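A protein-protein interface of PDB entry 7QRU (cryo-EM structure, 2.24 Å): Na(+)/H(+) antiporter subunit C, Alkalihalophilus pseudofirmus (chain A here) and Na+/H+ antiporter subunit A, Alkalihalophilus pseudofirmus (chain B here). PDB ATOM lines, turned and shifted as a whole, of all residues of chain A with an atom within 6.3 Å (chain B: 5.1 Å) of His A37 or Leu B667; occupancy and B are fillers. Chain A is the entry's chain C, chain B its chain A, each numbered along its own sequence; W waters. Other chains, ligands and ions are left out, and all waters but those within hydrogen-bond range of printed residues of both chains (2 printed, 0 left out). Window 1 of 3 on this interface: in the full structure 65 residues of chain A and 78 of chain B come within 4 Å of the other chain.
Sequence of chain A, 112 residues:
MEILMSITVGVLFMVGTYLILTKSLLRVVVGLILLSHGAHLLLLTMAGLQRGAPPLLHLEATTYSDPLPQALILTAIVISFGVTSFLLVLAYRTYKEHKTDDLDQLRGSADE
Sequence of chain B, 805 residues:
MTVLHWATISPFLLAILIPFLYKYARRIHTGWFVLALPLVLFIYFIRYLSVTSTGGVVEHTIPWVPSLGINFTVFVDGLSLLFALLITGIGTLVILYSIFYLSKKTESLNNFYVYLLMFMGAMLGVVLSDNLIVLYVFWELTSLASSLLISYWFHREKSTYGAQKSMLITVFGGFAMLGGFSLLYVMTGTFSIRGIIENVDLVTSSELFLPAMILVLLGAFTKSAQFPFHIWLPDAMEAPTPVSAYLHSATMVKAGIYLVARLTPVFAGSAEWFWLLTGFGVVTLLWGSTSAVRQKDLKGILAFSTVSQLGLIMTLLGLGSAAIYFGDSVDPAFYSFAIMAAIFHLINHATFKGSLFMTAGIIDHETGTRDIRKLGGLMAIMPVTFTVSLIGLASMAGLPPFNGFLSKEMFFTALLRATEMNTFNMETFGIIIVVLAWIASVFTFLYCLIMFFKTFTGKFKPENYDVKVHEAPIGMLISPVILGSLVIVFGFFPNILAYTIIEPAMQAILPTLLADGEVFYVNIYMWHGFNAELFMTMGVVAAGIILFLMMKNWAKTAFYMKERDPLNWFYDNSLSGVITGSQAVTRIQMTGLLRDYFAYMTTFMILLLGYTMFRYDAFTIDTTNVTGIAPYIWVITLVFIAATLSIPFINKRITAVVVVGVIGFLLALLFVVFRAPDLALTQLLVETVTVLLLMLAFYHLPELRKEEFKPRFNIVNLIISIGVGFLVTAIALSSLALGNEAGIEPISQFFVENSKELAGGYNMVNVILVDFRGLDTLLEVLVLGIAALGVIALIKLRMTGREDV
Water W1 lies within hydrogen-bond range of the side-chain carboxylate of Glu B687 (2.5 Å), a ring nitrogen (NE2) of His A37 (2.8 Å) and the backbone NH of Gly B664 (3.5 Å).
Water W2 lies within hydrogen-bond range of ND1 of His A40, ND1 of His A37 and NE2 of Gln B683.
The side-chain amide oxygen of Gln B683 lies close to the side-chain carboxylate of Glu B687 (2.7 Å).
Of the printed residues of chain B, Leu A12 touches Phe B640.
Of the printed residues of chain A, Phe B640 touches Leu A12 (3.7 Å).
Of the printed residues of chain A, Ile B663 touches His A37.
Of chain A, only His A37 (3.5 Å) comes within 4 Å of Leu B667.
Of the printed residues of chain A, Gln B683 touches His A37 (3.7 Å).
Printed residues of chain A within 4 Å of Glu B687: His A37 (3.7 Å).
The nearest printed residue of chain B that does not touch His A37 is Gly B664 (4.7 Å).
The nearest residue of chain A that does not touch Leu B667 is Leu A41 (4.2 Å).
The nearest printed residue of chain B that does not touch Leu A12 is Ile B663 (4.9 Å).
Hydrophobic or aromatic side chains of chain B that line the printed part of chain A: Phe B640, Ile B663 and Leu B667.
Among the printed residues, 5 pairs touch across the chains.
Among the printed residues, no Asp or Glu carboxylate lies within 4 Å of a Lys or Arg side-chain nitrogen of the other chain.
Phe B640 touches Leu A12.
Ile B663 touches His A37.
ND1 of His A37 touches CD2 of Leu B667, at 3.5 Å.
CE1 of His A37 touches OE1 of Gln B683 (3.7 Å).
Glu B687 touches His A37.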
ATOM      1  N   VAL A   9      12.175 -11.066   0.373  1.00  0.00           N
ATOM      2  CA  VAL A   9      11.176 -10.234   1.010  1.00  0.00           C
ATOM      3  C   VAL A   9      10.311  -9.574  -0.061  1.00  0.00           C
ATOM      4  O   VAL A   9       9.069  -9.536   0.055  1.00  0.00           O
ATOM      5  CB  VAL A   9      11.886  -9.229   1.945  1.00  0.00           C
ATOM      6  CG1 VAL A   9      10.967  -8.096   2.482  1.00  0.00           C
ATOM      7  CG2 VAL A   9      12.506  -9.971   3.128  1.00  0.00           C
ATOM      8  N   LEU A  12       7.683 -11.994  -1.155  1.00  0.00           N
ATOM      9  CA  LEU A  12       6.566 -12.064  -0.236  1.00  0.00           C
ATOM     10  C   LEU A  12       5.729 -10.782  -0.314  1.00  0.00           C
ATOM     11  O   LEU A  12       4.538 -10.850  -0.243  1.00  0.00           O
ATOM     12  CB  LEU A  12       7.073 -12.279   1.197  1.00  0.00           C
ATOM     13  CG  LEU A  12       7.672 -13.659   1.446  1.00  0.00           C
ATOM     14  CD1 LEU A  12       8.585 -13.669   2.624  1.00  0.00           C
ATOM     15  CD2 LEU A  12       6.539 -14.573   1.712  1.00  0.00           C
ATOM     16  N   PHE A  13       6.309  -9.600  -0.394  1.00  0.00           N
ATOM     17  CA  PHE A  13       5.483  -8.393  -0.465  1.00  0.00           C
ATOM     18  C   PHE A  13       4.680  -8.355  -1.734  1.00  0.00           C
ATOM     19  O   PHE A  13       3.485  -8.076  -1.707  1.00  0.00           O
ATOM     20  CB  PHE A  13       6.377  -7.162  -0.317  1.00  0.00           C
ATOM     21  CG  PHE A  13       6.356  -6.815   1.143  1.00  0.00           C
ATOM     22  CD1 PHE A  13       7.202  -7.457   2.030  1.00  0.00           C
ATOM     23  CD2 PHE A  13       5.419  -5.912   1.634  1.00  0.00           C
ATOM     24  CE1 PHE A  13       7.203  -7.118   3.375  1.00  0.00           C
ATOM     25  CE2 PHE A  13       5.351  -5.643   3.006  1.00  0.00           C
ATOM     26  CZ  PHE A  13       6.235  -6.271   3.881  1.00  0.00           C
ATOM     27  N   LEU A  32      -2.269 -11.349   4.094  1.00  0.00           N
ATOM     28  CA  LEU A  32      -1.837 -10.634   5.283  1.00  0.00           C
ATOM     29  C   LEU A  32      -0.848 -11.478   6.072  1.00  0.00           C
ATOM     30  O   LEU A  32       0.192 -10.924   6.427  1.00  0.00           O
ATOM     31  CB  LEU A  32      -3.034 -10.217   6.141  1.00  0.00           C
ATOM     32  CG  LEU A  32      -3.816  -9.014   5.581  1.00  0.00           C
ATOM     33  CD1 LEU A  32      -5.061  -8.811   6.413  1.00  0.00           C
ATOM     34  CD2 LEU A  32      -2.944  -7.772   5.532  1.00  0.00           C
ATOM     35  N   ILE A  33      -1.024 -12.808   6.112  1.00  0.00           N
ATOM     36  CA  ILE A  33      -0.008 -13.704   6.675  1.00  0.00           C
ATOM     37  C   ILE A  33       1.296 -13.697   5.876  1.00  0.00           C
ATOM     38  O   ILE A  33       2.357 -13.558   6.470  1.00  0.00           O
ATOM     39  CB  ILE A  33      -0.584 -15.107   6.746  1.00  0.00           C
ATOM     40  CG1 ILE A  33      -1.631 -15.209   7.827  1.00  0.00           C
ATOM     41  CG2 ILE A  33       0.490 -16.155   6.889  1.00  0.00           C
ATOM     42  CD1 ILE A  33      -2.475 -16.528   7.644  1.00  0.00           C
ATOM     43  N   LEU A  34       1.258 -13.688   4.540  1.00  0.00           N
ATOM     44  CA  LEU A  34       2.532 -13.556   3.888  1.00  0.00           C
ATOM     45  C   LEU A  34       3.244 -12.211   4.135  1.00  0.00           C
ATOM     46  O   LEU A  34       4.482 -12.156   4.165  1.00  0.00           O
ATOM     47  CB  LEU A  34       2.281 -13.750   2.392  1.00  0.00           C
ATOM     48  CG  LEU A  34       1.812 -15.106   1.913  1.00  0.00           C
ATOM     49  CD1 LEU A  34       1.786 -15.070   0.383  1.00  0.00           C
ATOM     50  CD2 LEU A  34       2.740 -16.184   2.343  1.00  0.00           C
ATOM     51  N   LEU A  35       2.511 -11.085   4.163  1.00  0.00           N
ATOM     52  CA  LEU A  35       3.178  -9.836   4.418  1.00  0.00           C
ATOM     53  C   LEU A  35       3.821  -9.883   5.808  1.00  0.00           C
ATOM     54  O   LEU A  35       4.944  -9.342   5.953  1.00  0.00           O
ATOM     55  CB  LEU A  35       2.218  -8.658   4.265  1.00  0.00           C
ATOM     56  CG  LEU A  35       1.625  -8.515   2.866  1.00  0.00           C
ATOM     57  CD1 LEU A  35       0.562  -7.462   2.801  1.00  0.00           C
ATOM     58  CD2 LEU A  35       2.700  -8.143   1.894  1.00  0.00           C
ATOM     59  N   SER A  36       3.159 -10.468   6.793  1.00  0.00           N
ATOM     60  CA  SER A  36       3.824 -10.533   8.084  1.00  0.00           C
ATOM     61  C   SER A  36       5.124 -11.320   7.948  1.00  0.00           C
ATOM     62  O   SER A  36       6.133 -10.830   8.457  1.00  0.00           O
ATOM     63  CB  SER A  36       2.963 -11.110   9.162  1.00  0.00           C
ATOM     64  OG  SER A  36       1.637 -10.563   9.096  1.00  0.00           O
ATOM     65  N   HIS A  37       5.114 -12.516   7.288  1.00  0.00           N
ATOM     66  CA  HIS A  37       6.352 -13.279   7.128  1.00  0.00           C
ATOM     67  C   HIS A  37       7.414 -12.432   6.492  1.00  0.00           C
ATOM     68  O   HIS A  37       8.544 -12.382   6.955  1.00  0.00           O
ATOM     69  CB  HIS A  37       6.210 -14.518   6.281  1.00  0.00           C
ATOM     70  CG  HIS A  37       5.421 -15.578   6.944  1.00  0.00           C
ATOM     71  ND1 HIS A  37       5.395 -15.736   8.276  1.00  0.00           N
ATOM     72  CD2 HIS A  37       4.646 -16.543   6.374  1.00  0.00           C
ATOM     73  CE1 HIS A  37       4.716 -16.846   8.531  1.00  0.00           C
ATOM     74  NE2 HIS A  37       4.179 -17.315   7.388  1.00  0.00           N
ATOM     75  N   GLY A  38       7.037 -11.720   5.438  1.00  0.00           N
ATOM     76  CA  GLY A  38       8.026 -10.844   4.856  1.00  0.00           C
ATOM     77  C   GLY A  38       8.615  -9.818   5.793  1.00  0.00           C
ATOM     78  O   GLY A  38       9.802  -9.481   5.681  1.00  0.00           O
ATOM     79  N   ALA A  39       7.776  -9.139   6.560  1.00  0.00           N
ATOM     80  CA  ALA A  39       8.296  -8.106   7.448  1.00  0.00           C
ATOM     81  C   ALA A  39       9.238  -8.724   8.481  1.00  0.00           C
ATOM     82  O   ALA A  39      10.326  -8.186   8.798  1.00  0.00           O
ATOM     83  CB  ALA A  39       7.156  -7.392   8.136  1.00  0.00           C
ATOM     84  N   HIS A  40       8.899  -9.905   8.937  1.00  0.00           N
ATOM     85  CA  HIS A  40       9.756 -10.510   9.937  1.00  0.00           C
ATOM     86  C   HIS A  40      11.065 -10.959   9.314  1.00  0.00           C
ATOM     87  O   HIS A  40      12.112 -10.720   9.877  1.00  0.00           O
ATOM     88  CB  HIS A  40       9.109 -11.742  10.519  1.00  0.00           C
ATOM     89  CG  HIS A  40       7.848 -11.464  11.241  1.00  0.00           C
ATOM     90  ND1 HIS A  40       6.830 -12.424  11.302  1.00  0.00           N
ATOM     91  CD2 HIS A  40       7.400 -10.250  11.763  1.00  0.00           C
ATOM     92  CE1 HIS A  40       5.774 -11.800  11.869  1.00  0.00           C
ATOM     93  NE2 HIS A  40       6.103 -10.467  12.152  1.00  0.00           N
ATOM     94  N   LEU A  41      11.032 -11.513   8.085  1.00  0.00           N
ATOM     95  CA  LEU A  41      12.291 -11.848   7.432  1.00  0.00           C
ATOM     96  C   LEU A  41      13.101 -10.600   7.109  1.00  0.00           C
ATOM     97  O   LEU A  41      14.295 -10.579   7.299  1.00  0.00           O
ATOM     98  CB  LEU A  41      11.987 -12.634   6.178  1.00  0.00           C
ATOM     99  CG  LEU A  41      13.173 -13.079   5.359  1.00  0.00           C
ATOM    100  CD1 LEU A  41      14.158 -13.928   6.164  1.00  0.00           C
ATOM    101  CD2 LEU A  41      12.624 -13.786   4.078  1.00  0.00           C
ATOM    102  N   LEU A  42      12.405  -9.460   6.822  1.00  0.00           N
ATOM    103  CA  LEU A  42      13.093  -8.205   6.549  1.00  0.00           C
ATOM    104  C   LEU A  42      13.847  -7.698   7.762  1.00  0.00           C
ATOM    105  O   LEU A  42      14.989  -7.239   7.681  1.00  0.00           O
ATOM    106  CB  LEU A  42      12.075  -7.195   6.038  1.00  0.00           C
ATOM    107  CG  LEU A  42      12.654  -5.824   5.699  1.00  0.00           C
ATOM    108  CD1 LEU A  42      13.629  -5.965   4.523  1.00  0.00           C
ATOM    109  CD2 LEU A  42      11.556  -4.821   5.371  1.00  0.00           C
ATOM    110  N   PHE B 640      11.403 -21.622  -1.624  1.00  0.00           N
ATOM    111  CA  PHE B 640      10.649 -20.656  -0.858  1.00  0.00           C
ATOM    112  C   PHE B 640       9.915 -19.696  -1.804  1.00  0.00           C
ATOM    113  O   PHE B 640       8.725 -19.386  -1.619  1.00  0.00           O
ATOM    114  CB  PHE B 640      11.624 -19.945   0.068  1.00  0.00           C
ATOM    115  CG  PHE B 640      10.944 -19.045   1.041  1.00  0.00           C
ATOM    116  CD1 PHE B 640      10.585 -17.773   0.684  1.00  0.00           C
ATOM    117  CD2 PHE B 640      10.551 -19.512   2.277  1.00  0.00           C
ATOM    118  CE1 PHE B 640       9.872 -16.979   1.565  1.00  0.00           C
ATOM    119  CE2 PHE B 640       9.913 -18.694   3.188  1.00  0.00           C
ATOM    120  CZ  PHE B 640       9.556 -17.431   2.815  1.00  0.00           C
ATOM    121  N   VAL B 662       4.259 -25.201   4.083  1.00  0.00           N
ATOM    122  CA  VAL B 662       5.557 -25.267   3.508  1.00  0.00           C
ATOM    123  C   VAL B 662       6.265 -23.955   3.798  1.00  0.00           C
ATOM    124  O   VAL B 662       7.465 -23.957   4.124  1.00  0.00           O
ATOM    125  CB  VAL B 662       5.557 -25.624   2.013  1.00  0.00           C
ATOM    126  CG1 VAL B 662       6.930 -25.381   1.413  1.00  0.00           C
ATOM    127  CG2 VAL B 662       5.079 -27.043   1.889  1.00  0.00           C
ATOM    128  N   ILE B 663       5.619 -22.847   3.495  1.00  0.00           N
ATOM    129  CA  ILE B 663       6.284 -21.550   3.621  1.00  0.00           C
ATOM    130  C   ILE B 663       6.724 -21.325   5.068  1.00  0.00           C
ATOM    131  O   ILE B 663       7.861 -20.881   5.332  1.00  0.00           O
ATOM    132  CB  ILE B 663       5.399 -20.400   3.056  1.00  0.00           C
ATOM    133  CG1 ILE B 663       5.527 -20.387   1.523  1.00  0.00           C
ATOM    134  CG2 ILE B 663       5.828 -19.081   3.611  1.00  0.00           C
ATOM    135  CD1 ILE B 663       4.286 -19.904   0.843  1.00  0.00           C
ATOM    136  N   GLY B 664       5.838 -21.626   5.998  1.00  0.00           N
ATOM    137  CA  GLY B 664       6.139 -21.587   7.419  1.00  0.00           C
ATOM    138  C   GLY B 664       7.305 -22.444   7.874  1.00  0.00           C
ATOM    139  O   GLY B 664       8.135 -21.999   8.621  1.00  0.00           O
ATOM    140  N   PHE B 665       7.367 -23.670   7.439  1.00  0.00           N
ATOM    141  CA  PHE B 665       8.500 -24.509   7.716  1.00  0.00           C
ATOM    142  C   PHE B 665       9.790 -23.970   7.124  1.00  0.00           C
ATOM    143  O   PHE B 665      10.853 -24.176   7.700  1.00  0.00           O
ATOM    144  CB  PHE B 665       8.355 -25.860   7.059  1.00  0.00           C
ATOM    145  CG  PHE B 665       7.634 -26.909   7.833  1.00  0.00           C
ATOM    146  CD1 PHE B 665       8.049 -27.267   9.111  1.00  0.00           C
ATOM    147  CD2 PHE B 665       6.651 -27.687   7.197  1.00  0.00           C
ATOM    148  CE1 PHE B 665       7.403 -28.308   9.777  1.00  0.00           C
ATOM    149  CE2 PHE B 665       5.960 -28.664   7.903  1.00  0.00           C
ATOM    150  CZ  PHE B 665       6.350 -28.983   9.181  1.00  0.00           C
ATOM    151  N   LEU B 666       9.745 -23.499   5.879  1.00  0.00           N
ATOM    152  CA  LEU B 666      10.952 -22.964   5.272  1.00  0.00           C
ATOM    153  C   LEU B 666      11.413 -21.663   5.942  1.00  0.00           C
ATOM    154  O   LEU B 666      12.603 -21.442   6.079  1.00  0.00           O
ATOM    155  CB  LEU B 666      10.807 -22.741   3.770  1.00  0.00           C
ATOM    156  CG  LEU B 666      10.909 -24.016   2.956  1.00  0.00           C
ATOM    157  CD1 LEU B 666      10.598 -23.758   1.496  1.00  0.00           C
ATOM    158  CD2 LEU B 666      12.260 -24.667   3.166  1.00  0.00           C
ATOM    159  N   LEU B 667      10.526 -20.798   6.344  1.00  0.00           N
ATOM    160  CA  LEU B 667      10.960 -19.631   7.099  1.00  0.00           C
ATOM    161  C   LEU B 667      11.607 -20.088   8.428  1.00  0.00           C
ATOM    162  O   LEU B 667      12.714 -19.693   8.749  1.00  0.00           O
ATOM    163  CB  LEU B 667       9.751 -18.696   7.230  1.00  0.00           C
ATOM    164  CG  LEU B 667      10.087 -17.367   7.833  1.00  0.00           C
ATOM    165  CD1 LEU B 667      10.940 -16.653   6.846  1.00  0.00           C
ATOM    166  CD2 LEU B 667       8.837 -16.550   8.225  1.00  0.00           C
ATOM    167  N   ALA B 668      11.119 -21.116   9.093  1.00  0.00           N
ATOM    168  CA  ALA B 668      11.836 -21.621  10.269  1.00  0.00           C
ATOM    169  C   ALA B 668      13.204 -22.144   9.905  1.00  0.00           C
ATOM    170  O   ALA B 668      14.185 -21.854  10.617  1.00  0.00           O
ATOM    171  CB  ALA B 668      11.048 -22.692  10.972  1.00  0.00           C
ATOM    172  N   LEU B 669      13.328 -22.843   8.781  1.00  0.00           N
ATOM    173  CA  LEU B 669      14.652 -23.292   8.334  1.00  0.00           C
ATOM    174  C   LEU B 669      15.606 -22.138   8.069  1.00  0.00           C
ATOM    175  O   LEU B 669      16.793 -22.180   8.379  1.00  0.00           O
ATOM    176  CB  LEU B 669      14.426 -24.105   7.059  1.00  0.00           C
ATOM    177  CG  LEU B 669      15.712 -24.642   6.424  1.00  0.00           C
ATOM    178  CD1 LEU B 669      16.458 -25.383   7.488  1.00  0.00           C
ATOM    179  CD2 LEU B 669      15.465 -25.551   5.239  1.00  0.00           C
ATOM    180  N   LEU B 670      15.136 -21.032   7.461  1.00  0.00           N
ATOM    181  CA  LEU B 670      16.002 -19.886   7.289  1.00  0.00           C
ATOM    182  C   LEU B 670      16.422 -19.336   8.641  1.00  0.00           C
ATOM    183  O   LEU B 670      17.563 -18.899   8.798  1.00  0.00           O
ATOM    184  CB  LEU B 670      15.265 -18.829   6.458  1.00  0.00           C
ATOM    185  CG  LEU B 670      15.047 -19.201   4.983  1.00  0.00           C
ATOM    186  CD1 LEU B 670      14.273 -18.097   4.344  1.00  0.00           C
ATOM    187  CD2 LEU B 670      16.344 -19.380   4.233  1.00  0.00           C
ATOM    188  N   PHE B 671      15.494 -19.272   9.621  1.00  0.00           N
ATOM    189  CA  PHE B 671      15.900 -18.752  10.910  1.00  0.00           C
ATOM    190  C   PHE B 671      17.035 -19.582  11.522  1.00  0.00           C
ATOM    191  O   PHE B 671      17.959 -18.982  12.098  1.00  0.00           O
ATOM    192  CB  PHE B 671      14.762 -18.656  11.915  1.00  0.00           C
ATOM    193  CG  PHE B 671      13.763 -17.598  11.574  1.00  0.00           C
ATOM    194  CD1 PHE B 671      14.153 -16.479  10.921  1.00  0.00           C
ATOM    195  CD2 PHE B 671      12.404 -17.782  11.818  1.00  0.00           C
ATOM    196  CE1 PHE B 671      13.219 -15.487  10.651  1.00  0.00           C
ATOM    197  CE2 PHE B 671      11.465 -16.818  11.488  1.00  0.00           C
ATOM    198  CZ  PHE B 671      11.894 -15.650  10.910  1.00  0.00           C
ATOM    199  N   GLN B 683       8.564 -19.718  15.450  1.00  0.00           N
ATOM    200  CA  GLN B 683       7.960 -19.728  14.153  1.00  0.00           C
ATOM    201  C   GLN B 683       7.285 -21.080  13.886  1.00  0.00           C
ATOM    202  O   GLN B 683       6.156 -21.120  13.459  1.00  0.00           O
ATOM    203  CB  GLN B 683       8.960 -19.332  13.086  1.00  0.00           C
ATOM    204  CG  GLN B 683       8.371 -19.381  11.671  1.00  0.00           C
ATOM    205  CD  GLN B 683       7.362 -18.273  11.521  1.00  0.00           C
ATOM    206  OE1 GLN B 683       6.161 -18.498  11.456  1.00  0.00           O
ATOM    207  NE2 GLN B 683       7.858 -17.044  11.603  1.00  0.00           N
ATOM    208  N   GLU B 687       3.274 -21.542  13.498  1.00  0.00           N
ATOM    209  CA  GLU B 687       2.771 -22.096  12.250  1.00  0.00           C
ATOM    210  C   GLU B 687       1.836 -23.294  12.490  1.00  0.00           C
ATOM    211  O   GLU B 687       0.769 -23.383  11.860  1.00  0.00           O
ATOM    212  CB  GLU B 687       3.944 -22.422  11.324  1.00  0.00           C
ATOM    213  CG  GLU B 687       4.470 -21.170  10.614  1.00  0.00           C
ATOM    214  CD  GLU B 687       3.510 -19.976  10.618  1.00  0.00           C
ATOM    215  OE1 GLU B 687       3.565 -19.181  11.591  1.00  0.00           O
ATOM    216  OE2 GLU B 687       2.688 -19.823   9.654  1.00  0.00           O
HETATM  217  O   HOH W   1       3.092 -19.860   7.211  1.00  0.00           O
HETATM  218  O   HOH W   2       6.665 -14.899  10.467  1.00  0.00           O
